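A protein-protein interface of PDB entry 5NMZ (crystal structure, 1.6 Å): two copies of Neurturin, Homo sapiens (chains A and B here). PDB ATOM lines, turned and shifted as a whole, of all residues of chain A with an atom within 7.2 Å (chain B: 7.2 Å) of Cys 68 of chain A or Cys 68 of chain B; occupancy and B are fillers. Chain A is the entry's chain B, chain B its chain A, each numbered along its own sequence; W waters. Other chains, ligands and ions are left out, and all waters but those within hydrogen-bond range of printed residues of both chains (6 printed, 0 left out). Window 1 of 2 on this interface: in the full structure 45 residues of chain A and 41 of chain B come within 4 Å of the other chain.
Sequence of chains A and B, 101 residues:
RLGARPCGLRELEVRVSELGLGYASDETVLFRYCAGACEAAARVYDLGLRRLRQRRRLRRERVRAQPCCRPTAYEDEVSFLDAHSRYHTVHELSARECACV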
ATOM      1  N   CYS A   7     -30.431  -9.692 -24.121  1.00  0.00           N
ATOM      2  CA  CYS A   7     -29.288  -9.199 -23.340  1.00  0.00           C
ATOM      3  C   CYS A   7     -28.187  -8.721 -24.261  1.00  0.00           C
ATOM      4  O   CYS A   7     -27.784  -9.438 -25.174  1.00  0.00           O
ATOM      5  CB  CYS A   7     -28.791 -10.315 -22.422  1.00  0.00           C
ATOM      6  SG  CYS A   7     -27.297  -9.911 -21.471  1.00  0.00           S
ATOM      7  N   GLY A  36     -31.190  -6.353 -20.746  1.00  0.00           N
ATOM      8  CA  GLY A  36     -31.986  -7.173 -21.644  1.00  0.00           C
ATOM      9  C   GLY A  36     -32.414  -8.517 -21.120  1.00  0.00           C
ATOM     10  O   GLY A  36     -32.050  -8.917 -20.012  1.00  0.00           O
ATOM     11  N   CYS A  38     -33.066 -12.717 -20.934  1.00  0.00           N
ATOM     12  CA  CYS A  38     -32.283 -13.914 -21.033  1.00  0.00           C
ATOM     13  C   CYS A  38     -33.125 -15.173 -21.292  1.00  0.00           C
ATOM     14  O   CYS A  38     -32.637 -16.265 -21.041  1.00  0.00           O
ATOM     15  CB  CYS A  38     -31.344 -14.065 -19.831  1.00  0.00           C
ATOM     16  SG  CYS A  38     -29.907 -12.951 -19.892  1.00  0.00           S
ATOM     17  N   ARG A  64     -29.955 -19.027  -7.732  1.00  0.00           N
ATOM     18  CA  ARG A  64     -30.413 -18.318  -8.920  1.00  0.00           C
ATOM     19  C   ARG A  64     -30.646 -19.375  -9.957  1.00  0.00           C
ATOM     20  O   ARG A  64     -29.681 -20.007 -10.405  1.00  0.00           O
ATOM     21  CB  ARG A  64     -29.318 -17.376  -9.437  1.00  0.00           C
ATOM     22  CG  ARG A  64     -28.837 -16.319  -8.457  1.00  0.00           C
ATOM     23  CD  ARG A  64     -29.851 -15.240  -8.340  1.00  0.00           C
ATOM     24  NE  ARG A  64     -29.284 -13.979  -7.884  1.00  0.00           N
ATOM     25  CZ  ARG A  64     -29.796 -12.807  -8.232  1.00  0.00           C
ATOM     26  NH1 ARG A  64     -30.794 -12.747  -9.102  1.00  0.00           N
ATOM     27  NH2 ARG A  64     -29.280 -11.682  -7.754  1.00  0.00           N
ATOM     28  N   GLN A  66     -32.287 -18.748 -12.816  1.00  0.00           N
ATOM     29  CA  GLN A  66     -32.522 -18.060 -14.101  1.00  0.00           C
ATOM     30  C   GLN A  66     -31.237 -17.310 -14.423  1.00  0.00           C
ATOM     31  O   GLN A  66     -30.629 -16.808 -13.472  1.00  0.00           O
ATOM     32  CB  GLN A  66     -33.660 -17.041 -13.986  1.00  0.00           C
ATOM     33  CG  GLN A  66     -35.030 -17.646 -14.129  1.00  0.00           C
ATOM     34  CD  GLN A  66     -36.059 -16.579 -13.907  1.00  0.00           C
ATOM     35  OE1 GLN A  66     -36.216 -16.064 -12.810  1.00  0.00           O
ATOM     36  NE2 GLN A  66     -36.820 -16.252 -14.936  1.00  0.00           N
ATOM     37  N   PRO A  67     -30.805 -17.244 -15.706  1.00  0.00           N
ATOM     38  CA  PRO A  67     -29.592 -16.472 -16.031  1.00  0.00           C
ATOM     39  C   PRO A  67     -29.798 -14.988 -15.782  1.00  0.00           C
ATOM     40  O   PRO A  67     -30.938 -14.486 -15.733  1.00  0.00           O
ATOM     41  CB  PRO A  67     -29.367 -16.763 -17.525  1.00  0.00           C
ATOM     42  CG  PRO A  67     -30.216 -17.985 -17.851  1.00  0.00           C
ATOM     43  CD  PRO A  67     -31.412 -17.817 -16.928  1.00  0.00           C
ATOM     44  N   CYS A  68     -28.691 -14.286 -15.547  1.00  0.00           N
ATOM     45  CA  CYS A  68     -28.671 -12.863 -15.306  1.00  0.00           C
ATOM     46  C   CYS A  68     -27.957 -12.250 -16.505  1.00  0.00           C
ATOM     47  O   CYS A  68     -26.890 -12.750 -16.871  1.00  0.00           O
ATOM     48  CB  CYS A  68     -27.877 -12.554 -14.033  1.00  0.00           C
ATOM     49  SG  CYS A  68     -28.729 -12.927 -12.482  1.00  0.00           S
ATOM     50  N   CYS A  69     -28.435 -11.116 -16.997  1.00  0.00           N
ATOM     51  CA  CYS A  69     -27.723 -10.388 -18.031  1.00  0.00           C
ATOM     52  C   CYS A  69     -26.683  -9.503 -17.324  1.00  0.00           C
ATOM     53  O   CYS A  69     -27.027  -8.566 -16.585  1.00  0.00           O
ATOM     54  CB  CYS A  69     -28.703  -9.579 -18.878  1.00  0.00           C
ATOM     55  SG  CYS A  69     -27.904  -8.531 -20.109  1.00  0.00           S
ATOM     56  N   ARG A  70     -25.395  -9.873 -17.457  1.00  0.00           N
ATOM     57  CA  ARG A  70     -24.347  -9.154 -16.733  1.00  0.00           C
ATOM     58  C   ARG A  70     -23.091  -8.962 -17.563  1.00  0.00           C
ATOM     59  O   ARG A  70     -22.869  -9.730 -18.526  1.00  0.00           O
ATOM     60  CB  ARG A  70     -23.944  -9.991 -15.476  1.00  0.00           C
ATOM     61  CG  ARG A  70     -24.985 -10.056 -14.376  1.00  0.00           C
ATOM     62  CD  ARG A  70     -25.030  -8.756 -13.612  1.00  0.00           C
ATOM     63  NE  ARG A  70     -23.801  -8.483 -12.851  1.00  0.00           N
ATOM     64  CZ  ARG A  70     -23.515  -7.318 -12.271  1.00  0.00           C
ATOM     65  NH1 ARG A  70     -24.335  -6.279 -12.405  1.00  0.00           N
ATOM     66  NH2 ARG A  70     -22.384  -7.165 -11.601  1.00  0.00           N
ATOM     67  N   PRO A  71     -22.176  -8.026 -17.174  1.00  0.00           N
ATOM     68  CA  PRO A  71     -20.914  -7.926 -17.910  1.00  0.00           C
ATOM     69  C   PRO A  71     -20.031  -9.140 -17.754  1.00  0.00           C
ATOM     70  O   PRO A  71     -19.972  -9.744 -16.677  1.00  0.00           O
ATOM     71  CB  PRO A  71     -20.213  -6.690 -17.319  1.00  0.00           C
ATOM     72  CG  PRO A  71     -21.352  -5.902 -16.657  1.00  0.00           C
ATOM     73  CD  PRO A  71     -22.248  -6.989 -16.119  1.00  0.00           C
ATOM     74  N   ALA A  99     -23.247 -10.994 -21.290  1.00  0.00           N
ATOM     75  CA  ALA A  99     -23.737 -12.349 -21.524  1.00  0.00           C
ATOM     76  C   ALA A  99     -24.845 -12.682 -20.574  1.00  0.00           C
ATOM     77  O   ALA A  99     -24.966 -12.048 -19.528  1.00  0.00           O
ATOM     78  CB  ALA A  99     -22.632 -13.368 -21.383  1.00  0.00           C
ATOM     79  N   CYS A 100     -25.631 -13.723 -20.920  1.00  0.00           N
ATOM     80  CA  CYS A 100     -26.631 -14.246 -20.036  1.00  0.00           C
ATOM     81  C   CYS A 100     -25.881 -15.300 -19.258  1.00  0.00           C
ATOM     82  O   CYS A 100     -25.467 -16.316 -19.820  1.00  0.00           O
ATOM     83  CB  CYS A 100     -27.770 -14.864 -20.829  1.00  0.00           C
ATOM     84  SG  CYS A 100     -28.892 -13.637 -21.540  1.00  0.00           S
ATOM     85  N   VAL A 101     -25.642 -15.033 -17.985  1.00  0.00           N
ATOM     86  CA  VAL A 101     -24.854 -15.940 -17.165  1.00  0.00           C
ATOM     87  C   VAL A 101     -25.795 -16.762 -16.281  1.00  0.00           C
ATOM     88  O   VAL A 101     -25.896 -17.995 -16.503  1.00  0.00           O
ATOM     89  CB  VAL A 101     -23.750 -15.159 -16.382  1.00  0.00           C
ATOM     90  CG1 VAL A 101     -22.909 -14.318 -17.339  1.00  0.00           C
ATOM     91  CG2 VAL A 101     -24.327 -14.252 -15.299  1.00  0.00           C
ATOM     92  OXT VAL A 101     -26.499 -16.135 -15.457  1.00  0.00           O
ATOM     93  N   CYS B   7     -21.235 -17.393  -2.196  1.00  0.00           N
ATOM     94  CA  CYS B   7     -21.420 -18.066  -3.473  1.00  0.00           C
ATOM     95  C   CYS B   7     -20.358 -19.142  -3.719  1.00  0.00           C
ATOM     96  O   CYS B   7     -19.156 -18.894  -3.596  1.00  0.00           O
ATOM     97  CB  CYS B   7     -21.398 -17.015  -4.576  1.00  0.00           C
ATOM     98  SG  CYS B   7     -21.565 -17.697  -6.244  1.00  0.00           S
ATOM     99  N   GLY B  36     -25.599 -19.418  -2.877  1.00  0.00           N
ATOM    100  CA  GLY B  36     -24.984 -18.538  -1.890  1.00  0.00           C
ATOM    101  C   GLY B  36     -25.093 -17.064  -2.200  1.00  0.00           C
ATOM    102  O   GLY B  36     -25.721 -16.666  -3.182  1.00  0.00           O
ATOM    103  N   CYS B  38     -23.703 -12.949  -2.656  1.00  0.00           N
ATOM    104  CA  CYS B  38     -22.737 -12.107  -3.361  1.00  0.00           C
ATOM    105  C   CYS B  38     -22.842 -10.746  -2.715  1.00  0.00           C
ATOM    106  O   CYS B  38     -23.953 -10.290  -2.437  1.00  0.00           O
ATOM    107  CB  CYS B  38     -23.071 -12.016  -4.849  1.00  0.00           C
ATOM    108  SG  CYS B  38     -22.757 -13.552  -5.747  1.00  0.00           S
ATOM    109  N   ARG B  64     -29.729  -5.567 -14.290  1.00  0.00           N
ATOM    110  CA  ARG B  64     -29.248  -6.221 -13.070  1.00  0.00           C
ATOM    111  C   ARG B  64     -28.108  -5.396 -12.564  1.00  0.00           C
ATOM    112  O   ARG B  64     -27.045  -5.337 -13.199  1.00  0.00           O
ATOM    113  CB  ARG B  64     -28.822  -7.673 -13.323  1.00  0.00           C
ATOM    114  CG  ARG B  64     -29.844  -8.577 -13.932  1.00  0.00           C
ATOM    115  CD  ARG B  64     -30.899  -9.036 -12.964  1.00  0.00           C
ATOM    116  NE  ARG B  64     -31.519 -10.269 -13.442  1.00  0.00           N
ATOM    117  CZ  ARG B  64     -31.921 -11.263 -12.663  1.00  0.00           C
ATOM    118  NH1 ARG B  64     -31.793 -11.173 -11.347  1.00  0.00           N
ATOM    119  NH2 ARG B  64     -32.452 -12.358 -13.193  1.00  0.00           N
ATOM    120  N   GLN B  66     -26.622  -5.804  -9.481  1.00  0.00           N
ATOM    121  CA  GLN B  66     -25.889  -6.480  -8.418  1.00  0.00           C
ATOM    122  C   GLN B  66     -25.348  -7.772  -9.026  1.00  0.00           C
ATOM    123  O   GLN B  66     -25.974  -8.327  -9.898  1.00  0.00           O
ATOM    124  CB  GLN B  66     -26.804  -6.791  -7.203  1.00  0.00           C
ATOM    125  CG  GLN B  66     -27.805  -7.968  -7.337  1.00  0.00           C
ATOM    126  CD  GLN B  66     -29.014  -7.763  -8.238  1.00  0.00           C
ATOM    127  OE1 GLN B  66     -29.296  -6.674  -8.735  1.00  0.00           O
ATOM    128  NE2 GLN B  66     -29.782  -8.827  -8.455  1.00  0.00           N
ATOM    129  N   PRO B  67     -24.224  -8.270  -8.539  1.00  0.00           N
ATOM    130  CA  PRO B  67     -23.738  -9.573  -9.031  1.00  0.00           C
ATOM    131  C   PRO B  67     -24.710 -10.726  -8.743  1.00  0.00           C
ATOM    132  O   PRO B  67     -25.497 -10.693  -7.781  1.00  0.00           O
ATOM    133  CB  PRO B  67     -22.424  -9.782  -8.282  1.00  0.00           C
ATOM    134  CG  PRO B  67     -22.048  -8.407  -7.724  1.00  0.00           C
ATOM    135  CD  PRO B  67     -23.337  -7.700  -7.512  1.00  0.00           C
ATOM    136  N   CYS B  68     -24.654 -11.751  -9.602  1.00  0.00           N
ATOM    137  CA  CYS B  68     -25.463 -12.970  -9.529  1.00  0.00           C
ATOM    138  C   CYS B  68     -24.547 -14.139  -9.259  1.00  0.00           C
ATOM    139  O   CYS B  68     -23.533 -14.238  -9.950  1.00  0.00           O
ATOM    140  CB  CYS B  68     -26.217 -13.207 -10.829  1.00  0.00           C
ATOM    141  SG  CYS B  68     -27.545 -11.999 -11.129  1.00  0.00           S
ATOM    142  N   CYS B  69     -24.952 -15.079  -8.378  1.00  0.00           N
ATOM    143  CA  CYS B  69     -24.142 -16.276  -8.093  1.00  0.00           C
ATOM    144  C   CYS B  69     -24.546 -17.283  -9.129  1.00  0.00           C
ATOM    145  O   CYS B  69     -25.665 -17.791  -9.088  1.00  0.00           O
ATOM    146  CB  CYS B  69     -24.384 -16.815  -6.690  1.00  0.00           C
ATOM    147  SG  CYS B  69     -23.483 -18.320  -6.342  1.00  0.00           S
ATOM    148  N   ARG B  70     -23.694 -17.515 -10.109  1.00  0.00           N
ATOM    149  CA  ARG B  70     -24.071 -18.397 -11.231  1.00  0.00           C
ATOM    150  C   ARG B  70     -22.877 -19.210 -11.714  1.00  0.00           C
ATOM    151  O   ARG B  70     -21.721 -18.831 -11.456  1.00  0.00           O
ATOM    152  CB  ARG B  70     -24.556 -17.543 -12.430  1.00  0.00           C
ATOM    153  CG  ARG B  70     -25.901 -16.871 -12.234  1.00  0.00           C
ATOM    154  CD  ARG B  70     -27.040 -17.856 -12.349  1.00  0.00           C
ATOM    155  NE  ARG B  70     -27.147 -18.430 -13.704  1.00  0.00           N
ATOM    156  CZ  ARG B  70     -27.988 -19.395 -14.032  1.00  0.00           C
ATOM    157  NH1 ARG B  70     -28.755 -19.954 -13.109  1.00  0.00           N
ATOM    158  NH2 ARG B  70     -28.047 -19.835 -15.280  1.00  0.00           N
ATOM    159  N   PRO B  71     -23.107 -20.288 -12.497  1.00  0.00           N
ATOM    160  CA  PRO B  71     -21.940 -21.038 -13.012  1.00  0.00           C
ATOM    161  C   PRO B  71     -21.085 -20.258 -14.001  1.00  0.00           C
ATOM    162  O   PRO B  71     -21.627 -19.458 -14.783  1.00  0.00           O
ATOM    163  CB  PRO B  71     -22.567 -22.252 -13.710  1.00  0.00           C
ATOM    164  CG  PRO B  71     -23.964 -22.356 -13.105  1.00  0.00           C
ATOM    165  CD  PRO B  71     -24.376 -20.930 -12.913  1.00  0.00           C
ATOM    166  N   ALA B  99     -19.216 -18.318  -9.613  1.00  0.00           N
ATOM    167  CA  ALA B  99     -18.695 -17.008  -9.267  1.00  0.00           C
ATOM    168  C   ALA B  99     -19.814 -16.022  -9.126  1.00  0.00           C
ATOM    169  O   ALA B  99     -20.927 -16.245  -9.609  1.00  0.00           O
ATOM    170  CB  ALA B  99     -17.716 -16.486 -10.331  1.00  0.00           C
ATOM    171  N   CYS B 100     -19.484 -14.878  -8.479  1.00  0.00           N
ATOM    172  CA  CYS B 100     -20.397 -13.765  -8.384  1.00  0.00           C
ATOM    173  C   CYS B 100     -20.094 -12.969  -9.594  1.00  0.00           C
ATOM    174  O   CYS B 100     -18.990 -12.372  -9.697  1.00  0.00           O
ATOM    175  CB  CYS B 100     -20.115 -12.960  -7.123  1.00  0.00           C
ATOM    176  SG  CYS B 100     -20.740 -13.757  -5.637  1.00  0.00           S
ATOM    177  N   VAL B 101     -21.046 -12.961 -10.538  1.00  0.00           N
ATOM    178  CA  VAL B 101     -20.803 -12.272 -11.796  1.00  0.00           C
ATOM    179  C   VAL B 101     -21.605 -10.958 -11.790  1.00  0.00           C
ATOM    180  O   VAL B 101     -20.980  -9.866 -11.840  1.00  0.00           O
ATOM    181  CB  VAL B 101     -21.173 -13.191 -13.001  1.00  0.00           C
ATOM    182  CG1 VAL B 101     -20.862 -12.505 -14.324  1.00  0.00           C
ATOM    183  CG2 VAL B 101     -20.446 -14.526 -12.906  1.00  0.00           C
ATOM    184  OXT VAL B 101     -22.839 -11.053 -11.677  1.00  0.00           O
HETATM  185  O   HOH W   1     -27.080 -19.146  -7.258  1.00  0.00           O
HETATM  186  O   HOH W   2     -26.994 -14.435  -6.345  1.00  0.00           O
HETATM  187  O   HOH W   3     -31.048 -10.443 -16.158  1.00  0.00           O
HETATM  188  O   HOH W   4     -19.499  -9.091 -14.041  1.00  0.00           O
HETATM  189  O   HOH W   5     -23.703 -19.615 -16.507  1.00  0.00           O
HETATM  190  O   HOH W   6     -28.722  -6.351 -16.851  1.00  0.00           O
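Arg 64 of chain A touches Pro 67 of chain B.
Arg 64 of chain A touches Cys 68 of chain B.
Cys 69 of chain B touches Arg 64 of chain A.
O of Gln 66 of chain A touches NH1 of Arg 70 of chain B, 3.7 Å away.
Pro 67 of chain A touches Arg 64 of chain B (O to NH2, 3.6 Å).
Pro 67 of chain A touches Arg 70 of chain B.
CB of Arg 64 of chain B touches O of Cys 69 of chain A (3.8 Å).
Gln 66 of chain B touches Arg 70 of chain A.
Pro 67 of chain B touches Arg 70 of chain A.
Val 101 of chain B touches Pro 71 of chain A.
NH1 of Arg 64 of chain B lies close to SG of Cys 68 of chain A (3.7 Å).
The guanidinium group of Arg 70 of chain A sits at hydrogen-bond distance from the backbone carbonyl oxygen of Arg 64 of chain B (3.0 Å).
The guanidinium group (NH2) of Arg 64 of chain A sits close to the side-chain amide nitrogen (NE2) of Gln 66 of chain B, at 3.0 Å.
SG of Cys 68 of chain B is disulfide-bonded to SG of Cys 68 of chain A, at 2.0 Å.
NH1 of Arg 70 of chain B is in hydrogen-bond range of O of Arg 64 of chain A.
NE of Arg 70 of chain B is in salt-bridge range of OXT of Val 101 of chain A (3.0 Å).
OXT of Val 101 of chain B is in salt-bridge range of NE of Arg 70 of chain A (3.0 Å).
The guanidinium group (NH1) of Arg 64 of chain B lies close to the guanidinium group (NH1) of Arg 64 of chain A, at 2.9 Å.
Cys 68 of chain A touches just these residues of chain B: Arg 64 and Cys 68.
Printed residues of chain B within 4 Å of Cys 69 of chain A: Arg 64.
Of the printed residues of chain B, Val 101 of chain A touches Arg 70 (3.0 Å).
Gly 36 of chain B touches none of the printed residues of chain A.
Printed residues of chain A within 4 Å of Pro 67 of chain B: Arg 64 (3.9 Å) and Arg 70 (3.7 Å).
Of chain A, only Arg 64 and Cys 68 come within 4 Å of Cys 68 of chain B.
Printed residues of chain A within 4 Å of Cys 69 of chain B: Arg 64.
Printed residues of chain A within 4 Å of Arg 70 of chain B: Arg 64 (2.9 Å), Gln 66 (3.7 Å), Pro 67 (3.8 Å) and Val 101 (3.0 Å).
Cys 100 of chain B touches none of the printed residues of chain A.
The nearest residue of chain A that does not touch Cys 68 of chain B is Arg 70 of chain A (4.6 Å).
Arg 64 of chain A touches Cys 68 of chain B, and with the chains exchanged Cys 68 of chain A touches Arg 64 of chain B.
Arg 64 of chain A touches Cys 69 of chain B, and with the chains exchanged Cys 69 of chain A touches Arg 64 of chain B.
Gln 66 of chain A touches Arg 70 of chain B, and with the chains exchanged Arg 70 of chain A touches Gln 66 of chain B.
Pro 71 of chain A touches Val 101 of chain B, but with the chains exchanged Val 101 of chain A does not touch Pro 71 of chain B (4.8 Å).
Of the 18 pairs that touch across the chains among the printed residues, 16 have their exchanged pair printed and touching as well.
Of the 13 printed residues of chain A, 8 touch a printed residue of chain B.
Among the printed residues, no Asp or Glu carboxylate lies within 4 Å of a Lys or Arg side-chain nitrogen of the other chain.
Water W1 lies within hydrogen-bond range of the backbone carbonyl oxygen (O) of Cys 69 of chain B and the backbone NH (N) of Arg 64 of chain A.
Water W5 lies within hydrogen-bond range of O of Pro 71 of chain B (2.7 Å) and O of Val 101 of chain A (2.7 Å).
Water W4 lies within hydrogen-bond range of the backbone carbonyl oxygen (O) of Pro 71 of chain A (2.8 Å) and the chain-end carboxylate (O) of Val 101 of chain B (2.8 Å).
Water W3 lies within hydrogen-bond range of NE of Arg 64 of chain B (2.8 Å) and N of Cys 69 of chain A (2.8 Å).
Water W2 bridges NE of Arg 64 of chain A (2.8 Å) and N of Cys 69 of chain B (3.0 Å).
Water W6 lies within hydrogen-bond range of the backbone carbonyl oxygen (O) of Cys 69 of chain A (2.8 Å) and the backbone NH (N) of Arg 64 of chain B (2.9 Å).
SG of Cys 7 of chain B is disulfide-bonded to SG of Cys 69 of chain B (2.0 Å).
The side-chain sulfur (SG) of Cys 38 of chain B sits at hydrogen-bond distance from the backbone NH (N) of Cys 69 of chain B, 3.8 Å away.
The backbone NH (N) of Cys 69 of chain A lies close to the side-chain sulfur (SG) of Cys 38 of chain A (3.7 Å).
The backbone NH (N) of Arg 70 of chain A is in hydrogen-bond range of the backbone carbonyl oxygen (O) of Ala 99 of chain A, 3.0 Å away.
The side-chain sulfur (SG) of Cys 38 of chain B forms a disulfide with the side-chain sulfur (SG) of Cys 100 of chain B (2.0 Å).
The side-chain sulfur of Cys 38 of chain A is disulfide-bonded to the side-chain sulfur of Cys 100 of chain A (2.1 Å).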
